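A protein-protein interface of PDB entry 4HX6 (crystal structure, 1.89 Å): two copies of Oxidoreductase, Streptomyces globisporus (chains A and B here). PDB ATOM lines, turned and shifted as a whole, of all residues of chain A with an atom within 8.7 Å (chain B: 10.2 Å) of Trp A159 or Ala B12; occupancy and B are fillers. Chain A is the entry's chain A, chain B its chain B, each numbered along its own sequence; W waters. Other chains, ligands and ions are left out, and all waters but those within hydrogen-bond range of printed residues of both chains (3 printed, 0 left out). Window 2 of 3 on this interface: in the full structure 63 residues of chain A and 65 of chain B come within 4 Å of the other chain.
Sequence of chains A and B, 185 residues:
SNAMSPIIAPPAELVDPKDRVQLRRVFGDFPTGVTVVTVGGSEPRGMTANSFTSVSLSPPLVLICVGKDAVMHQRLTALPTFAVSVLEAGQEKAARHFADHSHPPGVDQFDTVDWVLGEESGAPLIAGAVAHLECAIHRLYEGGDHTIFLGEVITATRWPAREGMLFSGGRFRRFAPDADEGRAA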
ATOM      1  N   VAL A  84      11.188   9.382 -12.972  1.00  0.00           N
ATOM      2  CA  VAL A  84       9.966  10.146 -13.151  1.00  0.00           C
ATOM      3  C   VAL A  84       9.540  10.724 -11.806  1.00  0.00           C
ATOM      4  O   VAL A  84       9.418   9.982 -10.829  1.00  0.00           O
ATOM      5  CB  VAL A  84       8.835   9.249 -13.651  1.00  0.00           C
ATOM      6  CG1 VAL A  84       7.515  10.038 -13.724  1.00  0.00           C
ATOM      7  CG2 VAL A  84       9.196   8.642 -15.026  1.00  0.00           C
ATOM      8  N   SER A  85       9.330  12.041 -11.755  1.00  0.00           N
ATOM      9  CA  SER A  85       8.795  12.691 -10.555  1.00  0.00           C
ATOM     10  C   SER A  85       7.396  13.206 -10.872  1.00  0.00           C
ATOM     11  O   SER A  85       7.242  14.090 -11.711  1.00  0.00           O
ATOM     12  CB  SER A  85       9.707  13.852 -10.121  1.00  0.00           C
ATOM     13  OG  SER A  85      10.999  13.365  -9.777  1.00  0.00           O
ATOM     14  N   VAL A  86       6.379  12.637 -10.228  1.00  0.00           N
ATOM     15  CA  VAL A  86       5.004  13.085 -10.444  1.00  0.00           C
ATOM     16  C   VAL A  86       4.757  14.316  -9.581  1.00  0.00           C
ATOM     17  O   VAL A  86       4.780  14.223  -8.358  1.00  0.00           O
ATOM     18  CB  VAL A  86       3.981  12.000 -10.074  1.00  0.00           C
ATOM     19  CG1 VAL A  86       2.567  12.542 -10.233  1.00  0.00           C
ATOM     20  CG2 VAL A  86       4.169  10.784 -10.945  1.00  0.00           C
ATOM     21  N   GLU A  88       3.408  17.516  -7.503  1.00  0.00           N
ATOM     22  CA  GLU A  88       2.331  17.879  -6.602  1.00  0.00           C
ATOM     23  C   GLU A  88       1.720  19.213  -7.024  1.00  0.00           C
ATOM     24  O   GLU A  88       2.342  19.978  -7.756  1.00  0.00           O
ATOM     25  CB  GLU A  88       2.882  17.957  -5.168  1.00  0.00           C
ATOM     26  CG  GLU A  88       1.833  18.205  -4.077  1.00  0.00           C
ATOM     27  CD  GLU A  88       1.640  19.677  -3.746  1.00  0.00           C
ATOM     28  OE1 GLU A  88       2.450  20.522  -4.194  1.00  0.00           O
ATOM     29  OE2 GLU A  88       0.672  19.990  -3.024  1.00  0.00           O
ATOM     30  N   VAL A 116      16.826  15.169  -4.796  1.00  0.00           N
ATOM     31  CA  VAL A 116      17.678  14.170  -4.170  1.00  0.00           C
ATOM     32  C   VAL A 116      18.116  13.190  -5.242  1.00  0.00           C
ATOM     33  O   VAL A 116      17.379  12.927  -6.205  1.00  0.00           O
ATOM     34  CB  VAL A 116      16.951  13.418  -3.044  1.00  0.00           C
ATOM     35  CG1 VAL A 116      16.664  14.353  -1.887  1.00  0.00           C
ATOM     36  CG2 VAL A 116      15.664  12.816  -3.574  1.00  0.00           C
ATOM     37  N   LEU A 125      15.839  13.340  -8.379  1.00  0.00           N
ATOM     38  CA  LEU A 125      14.421  13.148  -8.117  1.00  0.00           C
ATOM     39  C   LEU A 125      13.926  14.452  -7.530  1.00  0.00           C
ATOM     40  O   LEU A 125      14.592  15.056  -6.705  1.00  0.00           O
ATOM     41  CB  LEU A 125      14.195  12.003  -7.118  1.00  0.00           C
ATOM     42  CG  LEU A 125      14.570  10.596  -7.601  1.00  0.00           C
ATOM     43  CD1 LEU A 125      14.425   9.556  -6.496  1.00  0.00           C
ATOM     44  CD2 LEU A 125      13.696  10.239  -8.783  1.00  0.00           C
ATOM     45  N   ILE A 126      12.753  14.891  -7.946  1.00  0.00           N
ATOM     46  CA  ILE A 126      12.288  16.195  -7.517  1.00  0.00           C
ATOM     47  C   ILE A 126      11.656  16.112  -6.137  1.00  0.00           C
ATOM     48  O   ILE A 126      10.676  15.390  -5.954  1.00  0.00           O
ATOM     49  CB  ILE A 126      11.263  16.766  -8.500  1.00  0.00           C
ATOM     50  CG1 ILE A 126      11.842  16.788  -9.918  1.00  0.00           C
ATOM     51  CG2 ILE A 126      10.857  18.156  -8.069  1.00  0.00           C
ATOM     52  CD1 ILE A 126      13.038  17.722 -10.091  1.00  0.00           C
ATOM     53  N   ALA A 127      12.222  16.849  -5.176  1.00  0.00           N
ATOM     54  CA  ALA A 127      11.695  16.874  -3.808  1.00  0.00           C
ATOM     55  C   ALA A 127      10.274  17.419  -3.795  1.00  0.00           C
ATOM     56  O   ALA A 127       9.958  18.322  -4.556  1.00  0.00           O
ATOM     57  CB  ALA A 127      12.589  17.726  -2.900  1.00  0.00           C
ATOM     58  N   GLY A 128       9.421  16.870  -2.936  1.00  0.00           N
ATOM     59  CA  GLY A 128       8.067  17.377  -2.788  1.00  0.00           C
ATOM     60  C   GLY A 128       7.041  16.775  -3.739  1.00  0.00           C
ATOM     61  O   GLY A 128       5.863  17.156  -3.723  1.00  0.00           O
ATOM     62  N   ALA A 129       7.483  15.827  -4.560  1.00  0.00           N
ATOM     63  CA  ALA A 129       6.621  15.210  -5.565  1.00  0.00           C
ATOM     64  C   ALA A 129       5.632  14.249  -4.917  1.00  0.00           C
ATOM     65  O   ALA A 129       5.836  13.807  -3.780  1.00  0.00           O
ATOM     66  CB  ALA A 129       7.478  14.454  -6.590  1.00  0.00           C
ATOM     67  N   VAL A 130       4.566  13.927  -5.644  1.00  0.00           N
ATOM     68  CA  VAL A 130       3.594  12.938  -5.187  1.00  0.00           C
ATOM     69  C   VAL A 130       4.203  11.536  -5.179  1.00  0.00           C
ATOM     70  O   VAL A 130       3.897  10.699  -4.307  1.00  0.00           O
ATOM     71  CB  VAL A 130       2.367  12.917  -6.119  1.00  0.00           C
ATOM     72  CG1 VAL A 130       1.385  11.847  -5.668  1.00  0.00           C
ATOM     73  CG2 VAL A 130       1.701  14.278  -6.152  1.00  0.00           C
ATOM     74  N   ALA A 131       5.042  11.279  -6.179  1.00  0.00           N
ATOM     75  CA  ALA A 131       5.698   9.982  -6.332  1.00  0.00           C
ATOM     76  C   ALA A 131       6.984  10.101  -7.132  1.00  0.00           C
ATOM     77  O   ALA A 131       7.148  11.017  -7.948  1.00  0.00           O
ATOM     78  CB  ALA A 131       4.753   8.962  -6.986  1.00  0.00           C
ATOM     79  N   HIS A 132       7.903   9.176  -6.881  1.00  0.00           N
ATOM     80  CA  HIS A 132       9.119   9.039  -7.672  1.00  0.00           C
ATOM     81  C   HIS A 132       9.134   7.632  -8.238  1.00  0.00           C
ATOM     82  O   HIS A 132       8.848   6.677  -7.511  1.00  0.00           O
ATOM     83  CB  HIS A 132      10.357   9.173  -6.795  1.00  0.00           C
ATOM     84  CG  HIS A 132      10.585  10.549  -6.247  1.00  0.00           C
ATOM     85  ND1 HIS A 132      11.225  10.768  -5.046  1.00  0.00           N
ATOM     86  CD2 HIS A 132      10.300  11.774  -6.747  1.00  0.00           C
ATOM     87  CE1 HIS A 132      11.297  12.068  -4.816  1.00  0.00           C
ATOM     88  NE2 HIS A 132      10.745  12.701  -5.835  1.00  0.00           N
ATOM     89  N   LEU A 133       9.480   7.499  -9.515  1.00  0.00           N
ATOM     90  CA  LEU A 133       9.694   6.193 -10.137  1.00  0.00           C
ATOM     91  C   LEU A 133      11.081   6.159 -10.782  1.00  0.00           C
ATOM     92  O   LEU A 133      11.457   7.077 -11.511  1.00  0.00           O
ATOM     93  CB  LEU A 133       8.638   5.918 -11.213  1.00  0.00           C
ATOM     94  CG  LEU A 133       7.178   5.811 -10.746  1.00  0.00           C
ATOM     95  CD1 LEU A 133       6.536   7.189 -10.592  1.00  0.00           C
ATOM     96  CD2 LEU A 133       6.367   4.970 -11.712  1.00  0.00           C
ATOM     97  N   ALA A 156      10.173   2.571  -6.637  1.00  0.00           N
ATOM     98  CA  ALA A 156       9.266   3.692  -6.574  1.00  0.00           C
ATOM     99  C   ALA A 156       8.968   4.057  -5.131  1.00  0.00           C
ATOM    100  O   ALA A 156       9.051   3.222  -4.232  1.00  0.00           O
ATOM    101  CB  ALA A 156       7.991   3.386  -7.343  1.00  0.00           C
ATOM    102  N   THR A 157       8.643   5.325  -4.926  1.00  0.00           N
ATOM    103  CA  THR A 157       8.262   5.834  -3.620  1.00  0.00           C
ATOM    104  C   THR A 157       7.069   6.743  -3.813  1.00  0.00           C
ATOM    105  O   THR A 157       6.972   7.418  -4.839  1.00  0.00           O
ATOM    106  CB  THR A 157       9.388   6.640  -2.996  1.00  0.00           C
ATOM    107  OG1 THR A 157      10.534   5.795  -2.830  1.00  0.00           O
ATOM    108  CG2 THR A 157       8.953   7.144  -1.640  1.00  0.00           C
ATOM    109  N   ARG A 158       6.152   6.763  -2.850  1.00  0.00           N
ATOM    110  CA  ARG A 158       5.013   7.669  -2.954  1.00  0.00           C
ATOM    111  C   ARG A 158       4.668   8.361  -1.639  1.00  0.00           C
ATOM    112  O   ARG A 158       4.963   7.842  -0.550  1.00  0.00           O
ATOM    113  CB  ARG A 158       3.783   6.939  -3.498  1.00  0.00           C
ATOM    114  CG  ARG A 158       3.247   5.864  -2.580  1.00  0.00           C
ATOM    115  CD  ARG A 158       2.108   5.096  -3.237  1.00  0.00           C
ATOM    116  NE  ARG A 158       0.973   5.949  -3.585  1.00  0.00           N
ATOM    117  CZ  ARG A 158      -0.166   5.993  -2.902  1.00  0.00           C
ATOM    118  NH1 ARG A 158      -0.330   5.241  -1.817  1.00  0.00           N
ATOM    119  NH2 ARG A 158      -1.145   6.788  -3.300  1.00  0.00           N
ATOM    120  N   TRP A 159       4.052   9.537  -1.767  1.00  0.00           N
ATOM    121  CA  TRP A 159       3.573  10.321  -0.634  1.00  0.00           C
ATOM    122  C   TRP A 159       2.047  10.438  -0.743  1.00  0.00           C
ATOM    123  O   TRP A 159       1.533  11.312  -1.416  1.00  0.00           O
ATOM    124  CB  TRP A 159       4.240  11.708  -0.622  1.00  0.00           C
ATOM    125  CG  TRP A 159       5.704  11.664  -0.251  1.00  0.00           C
ATOM    126  CD1 TRP A 159       6.247  11.937   0.971  1.00  0.00           C
ATOM    127  CD2 TRP A 159       6.803  11.281  -1.097  1.00  0.00           C
ATOM    128  NE1 TRP A 159       7.611  11.774   0.935  1.00  0.00           N
ATOM    129  CE2 TRP A 159       7.978  11.362  -0.317  1.00  0.00           C
ATOM    130  CE3 TRP A 159       6.907  10.892  -2.435  1.00  0.00           C
ATOM    131  CZ2 TRP A 159       9.243  11.079  -0.835  1.00  0.00           C
ATOM    132  CZ3 TRP A 159       8.166  10.602  -2.948  1.00  0.00           C
ATOM    133  CH2 TRP A 159       9.317  10.698  -2.149  1.00  0.00           C
ATOM    134  N   PRO A 160       1.322   9.519  -0.095  1.00  0.00           N
ATOM    135  CA  PRO A 160      -0.140   9.427  -0.198  1.00  0.00           C
ATOM    136  C   PRO A 160      -0.869  10.736   0.159  1.00  0.00           C
ATOM    137  O   PRO A 160      -1.918  11.023  -0.413  1.00  0.00           O
ATOM    138  CB  PRO A 160      -0.501   8.331   0.819  1.00  0.00           C
ATOM    139  CG  PRO A 160       0.732   7.521   0.964  1.00  0.00           C
ATOM    140  CD  PRO A 160       1.896   8.465   0.758  1.00  0.00           C
ATOM    141  N   ALA A 161      -0.327  11.519   1.083  1.00  0.00           N
ATOM    142  CA  ALA A 161      -0.990  12.760   1.489  1.00  0.00           C
ATOM    143  C   ALA A 161      -0.879  13.870   0.438  1.00  0.00           C
ATOM    144  O   ALA A 161      -1.538  14.897   0.553  1.00  0.00           O
ATOM    145  CB  ALA A 161      -0.458  13.241   2.829  1.00  0.00           C
ATOM    146  N   ARG A 162      -0.049  13.659  -0.578  1.00  0.00           N
ATOM    147  CA  ARG A 162       0.125  14.655  -1.632  1.00  0.00           C
ATOM    148  C   ARG A 162      -0.763  14.346  -2.833  1.00  0.00           C
ATOM    149  O   ARG A 162      -1.008  13.187  -3.158  1.00  0.00           O
ATOM    150  CB  ARG A 162       1.591  14.752  -2.063  1.00  0.00           C
ATOM    151  CG  ARG A 162       2.519  15.242  -0.962  1.00  0.00           C
ATOM    152  CD  ARG A 162       3.989  15.167  -1.358  1.00  0.00           C
ATOM    153  NE  ARG A 162       4.838  15.557  -0.233  1.00  0.00           N
ATOM    154  CZ  ARG A 162       6.156  15.392  -0.186  1.00  0.00           C
ATOM    155  NH1 ARG A 162       6.830  15.779   0.895  1.00  0.00           N
ATOM    156  NH2 ARG A 162       6.804  14.836  -1.209  1.00  0.00           N
ATOM    157  N   GLU A 163      -1.247  15.396  -3.480  1.00  0.00           N
ATOM    158  CA  GLU A 163      -2.153  15.248  -4.603  1.00  0.00           C
ATOM    159  C   GLU A 163      -1.488  15.843  -5.828  1.00  0.00           C
ATOM    160  O   GLU A 163      -0.838  16.877  -5.739  1.00  0.00           O
ATOM    161  CB  GLU A 163      -3.456  15.984  -4.307  1.00  0.00           C
ATOM    162  CG  GLU A 163      -4.641  15.546  -5.140  1.00  0.00           C
ATOM    163  CD  GLU A 163      -5.929  16.204  -4.671  1.00  0.00           C
ATOM    164  OE1 GLU A 163      -6.831  15.476  -4.200  1.00  0.00           O
ATOM    165  OE2 GLU A 163      -6.029  17.451  -4.764  1.00  0.00           O
ATOM    166  N   GLY A 164      -1.653  15.184  -6.970  1.00  0.00           N
ATOM    167  CA  GLY A 164      -0.974  15.591  -8.181  1.00  0.00           C
ATOM    168  C   GLY A 164      -1.474  16.854  -8.841  1.00  0.00           C
ATOM    169  O   GLY A 164      -2.645  17.227  -8.744  1.00  0.00           O
ATOM    170  N   PRO B  11       4.694  11.094   5.514  1.00  0.00           N
ATOM    171  CA  PRO B  11       5.796  10.133   5.374  1.00  0.00           C
ATOM    172  C   PRO B  11       5.836   9.470   3.999  1.00  0.00           C
ATOM    173  O   PRO B  11       4.814   9.376   3.305  1.00  0.00           O
ATOM    174  CB  PRO B  11       5.490   9.085   6.451  1.00  0.00           C
ATOM    175  CG  PRO B  11       4.020   9.212   6.701  1.00  0.00           C
ATOM    176  CD  PRO B  11       3.725  10.677   6.542  1.00  0.00           C
ATOM    177  N   ALA B  12       7.023   9.006   3.618  1.00  0.00           N
ATOM    178  CA  ALA B  12       7.207   8.332   2.337  1.00  0.00           C
ATOM    179  C   ALA B  12       6.891   6.844   2.433  1.00  0.00           C
ATOM    180  O   ALA B  12       7.345   6.140   3.342  1.00  0.00           O
ATOM    181  CB  ALA B  12       8.621   8.541   1.830  1.00  0.00           C
ATOM    182  N   GLU B  13       6.098   6.375   1.484  1.00  0.00           N
ATOM    183  CA  GLU B  13       5.732   4.975   1.400  1.00  0.00           C
ATOM    184  C   GLU B  13       6.557   4.323   0.289  1.00  0.00           C
ATOM    185  O   GLU B  13       6.455   4.691  -0.881  1.00  0.00           O
ATOM    186  CB  GLU B  13       4.237   4.869   1.113  1.00  0.00           C
ATOM    187  CG  GLU B  13       3.769   3.532   0.608  1.00  0.00           C
ATOM    188  CD  GLU B  13       2.283   3.534   0.300  1.00  0.00           C
ATOM    189  OE1 GLU B  13       1.511   4.114   1.097  1.00  0.00           O
ATOM    190  OE2 GLU B  13       1.890   2.955  -0.736  1.00  0.00           O
ATOM    191  N   LEU B  14       7.401   3.377   0.673  1.00  0.00           N
ATOM    192  CA  LEU B  14       8.235   2.656  -0.279  1.00  0.00           C
ATOM    193  C   LEU B  14       7.382   1.658  -1.062  1.00  0.00           C
ATOM    194  O   LEU B  14       6.535   0.975  -0.492  1.00  0.00           O
ATOM    195  CB  LEU B  14       9.359   1.943   0.482  1.00  0.00           C
ATOM    196  CG  LEU B  14      10.489   1.216  -0.248  1.00  0.00           C
ATOM    197  CD1 LEU B  14      10.983   1.999  -1.460  1.00  0.00           C
ATOM    198  CD2 LEU B  14      11.629   0.941   0.733  1.00  0.00           C
ATOM    199  N   VAL B  15       7.598   1.584  -2.372  1.00  0.00           N
ATOM    200  CA  VAL B  15       6.838   0.664  -3.209  1.00  0.00           C
ATOM    201  C   VAL B  15       7.723  -0.397  -3.845  1.00  0.00           C
ATOM    202  O   VAL B  15       8.720  -0.082  -4.486  1.00  0.00           O
ATOM    203  CB  VAL B  15       6.117   1.398  -4.343  1.00  0.00           C
ATOM    204  CG1 VAL B  15       5.538   0.393  -5.343  1.00  0.00           C
ATOM    205  CG2 VAL B  15       5.037   2.317  -3.784  1.00  0.00           C
ATOM    206  N   GLN B  22       0.759  -2.614  -4.451  1.00  0.00           N
ATOM    207  CA  GLN B  22       1.516  -1.385  -4.222  1.00  0.00           C
ATOM    208  C   GLN B  22       1.779  -0.633  -5.534  1.00  0.00           C
ATOM    209  O   GLN B  22       1.726   0.592  -5.578  1.00  0.00           O
ATOM    210  CB  GLN B  22       2.846  -1.678  -3.516  1.00  0.00           C
ATOM    211  CG  GLN B  22       2.723  -2.442  -2.201  1.00  0.00           C
ATOM    212  CD  GLN B  22       4.073  -2.822  -1.608  1.00  0.00           C
ATOM    213  OE1 GLN B  22       5.075  -2.143  -1.829  1.00  0.00           O
ATOM    214  NE2 GLN B  22       4.103  -3.918  -0.853  1.00  0.00           N
ATOM    215  N   ARG B  25      -1.125   1.363  -6.730  1.00  0.00           N
ATOM    216  CA  ARG B  25      -1.276   2.598  -5.968  1.00  0.00           C
ATOM    217  C   ARG B  25      -0.429   3.713  -6.552  1.00  0.00           C
ATOM    218  O   ARG B  25      -0.884   4.843  -6.666  1.00  0.00           O
ATOM    219  CB  ARG B  25      -0.958   2.395  -4.483  1.00  0.00           C
ATOM    220  CG  ARG B  25      -1.992   1.571  -3.748  1.00  0.00           C
ATOM    221  CD  ARG B  25      -1.917   1.819  -2.249  1.00  0.00           C
ATOM    222  NE  ARG B  25      -0.682   1.301  -1.671  1.00  0.00           N
ATOM    223  CZ  ARG B  25      -0.604   0.163  -0.992  1.00  0.00           C
ATOM    224  NH1 ARG B  25       0.560  -0.242  -0.499  1.00  0.00           N
ATOM    225  NH2 ARG B  25      -1.695  -0.566  -0.800  1.00  0.00           N
ATOM    226  N   VAL B  26       0.802   3.406  -6.940  1.00  0.00           N
ATOM    227  CA  VAL B  26       1.652   4.458  -7.467  1.00  0.00           C
ATOM    228  C   VAL B  26       1.212   4.875  -8.890  1.00  0.00           C
ATOM    229  O   VAL B  26       1.267   6.051  -9.244  1.00  0.00           O
ATOM    230  CB  VAL B  26       3.168   4.089  -7.392  1.00  0.00           C
ATOM    231  CG1 VAL B  26       3.529   3.033  -8.413  1.00  0.00           C
ATOM    232  CG2 VAL B  26       4.029   5.341  -7.603  1.00  0.00           C
ATOM    233  N   GLY B  28      -1.739   4.896  -9.850  1.00  0.00           N
ATOM    234  CA  GLY B  28      -2.912   5.716  -9.579  1.00  0.00           C
ATOM    235  C   GLY B  28      -2.603   7.161  -9.199  1.00  0.00           C
ATOM    236  O   GLY B  28      -3.511   7.992  -9.155  1.00  0.00           O
ATOM    237  N   ASP B  29      -1.338   7.466  -8.910  1.00  0.00           N
ATOM    238  CA  ASP B  29      -0.960   8.811  -8.448  1.00  0.00           C
ATOM    239  C   ASP B  29      -0.828   9.801  -9.602  1.00  0.00           C
ATOM    240  O   ASP B  29      -0.826  11.014  -9.391  1.00  0.00           O
ATOM    241  CB  ASP B  29       0.349   8.784  -7.656  1.00  0.00           C
ATOM    242  CG  ASP B  29       0.203   8.147  -6.286  1.00  0.00           C
ATOM    243  OD1 ASP B  29      -0.912   8.146  -5.710  1.00  0.00           O
ATOM    244  OD2 ASP B  29       1.228   7.663  -5.769  1.00  0.00           O
ATOM    245  N   PHE B  30      -0.723   9.284 -10.825  1.00  0.00           N
ATOM    246  CA  PHE B  30      -0.740  10.147 -12.003  1.00  0.00           C
ATOM    247  C   PHE B  30      -2.171  10.299 -12.522  1.00  0.00           C
ATOM    248  O   PHE B  30      -2.763   9.343 -13.009  1.00  0.00           O
ATOM    249  CB  PHE B  30       0.160   9.563 -13.094  1.00  0.00           C
ATOM    250  CG  PHE B  30       0.321  10.454 -14.299  1.00  0.00           C
ATOM    251  CD1 PHE B  30       1.174  11.548 -14.262  1.00  0.00           C
ATOM    252  CD2 PHE B  30      -0.368  10.183 -15.472  1.00  0.00           C
ATOM    253  CE1 PHE B  30       1.333  12.358 -15.377  1.00  0.00           C
ATOM    254  CE2 PHE B  30      -0.221  10.989 -16.581  1.00  0.00           C
ATOM    255  CZ  PHE B  30       0.638  12.077 -16.535  1.00  0.00           C
HETATM  256  O   HOH W   1       2.237  11.361   2.450  1.00  0.00           O
HETATM  257  O   HOH W   2      -2.137  12.300  -7.493  1.00  0.00           O
HETATM  258  O   HOH W   3      -2.098   3.489   0.438  1.00  0.00           O
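OE2 of Glu B13 lies within salt-bridge range of NH1 of Arg A158, 3.4 Å away.
O of Ala A156 lies within hydrogen-bond range of N of Val B15.
The guanidinium group (NH2) of Arg A158 is in salt-bridge range of the side-chain carboxylate (OD1) of Asp B29.
The backbone NH (N) of His A132 is in hydrogen-bond range of the backbone carbonyl oxygen (O) of Thr A157.
The side-chain carboxylate (OE2) of Glu B13 lies within salt-bridge range of the guanidinium group (NE) of Arg B25 (3.2 Å).
The backbone carbonyl oxygen of Ala A131 lies within hydrogen-bond range of the backbone NH of Val A86.
N of Trp A159 lies within hydrogen-bond range of O of Val A130, at 2.8 Å.
N of Val A130 lies within hydrogen-bond range of O of Val A86.
Asp B29 touches Val A86 (O to CG1, 3.8 Å).
Asp B29 touches Val A130.
CB of Ala A131 touches CG2 of Val B26, 3.7 Å away.
Ala A156 touches Leu B14.
Ala B12 touches Thr A157.
Glu B13 touches Thr A157 (O to CA, 3.5 Å).
CA of Ala B12 touches O of Arg A158 (3.7 Å).
Pro B11 touches Trp A159 (O to CD1, 3.7 Å).
NE1 of Trp A159 touches CB of Ala B12, at 3.5 Å.
Pro A160 touches Glu B13 (CG to OE1, 3.5 Å).
Ala A131 touches two residues of chain B.
Of the printed residues of chain B, Ala A156 touches Leu B14 (3.6 Å) and Val B15 (2.9 Å).
Trp A159 touches two residues of chain B.
Printed residues of chain B within 4 Å of Pro A160: Pro B11 and Glu B13.
Ala A161 touches none of the printed residues of chain B.
No residue of chain B comes within 4 Å of Arg A162.
Of chain A, only Thr A157, Arg A158 and Trp A159 come within 4 Å of Ala B12.
Of the printed residues of chain A, Arg B25 touches Arg A158.
The nearest residue of chain B that does not touch Trp A159 is Glu B13 (5.0 Å).
The nearest residue of chain A that does not touch Ala B12 is Pro A160 (5.5 Å).
Of the 11 printed residues of chain B, 8 touch a printed residue of chain A.
Hydrophobic or aromatic side chains of chain B that line the printed part of chain A: Ala B12, Leu B14, Val B15 and Val B26.
Of the 23 printed residues of chain A, 8 touch a printed residue of chain B.
Hydrophobic or aromatic side chains of chain A that line the printed part of chain B: Val A86, Val A130, Ala A131, Trp A159 and Pro A160.
Among the printed residues, Asp or Glu carboxylates within 4 Å of a Lys or Arg side-chain nitrogen of the other chain: Arg A158 with Glu B13 (3.4 Å) and Arg A158 with Asp B29 (2.8 Å).
No position is printed for both chains.
Water W2 bridges the backbone carbonyl oxygen of Asp B29 and the backbone NH of Gly A164.
Water W1 lies within hydrogen-bond range of the backbone NH of Ala A161 (2.9 Å) and the backbone carbonyl oxygen of Pro B11 (3.4 Å).
Water W3 bridges NE of Arg B25 and NH1 of Arg A158.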
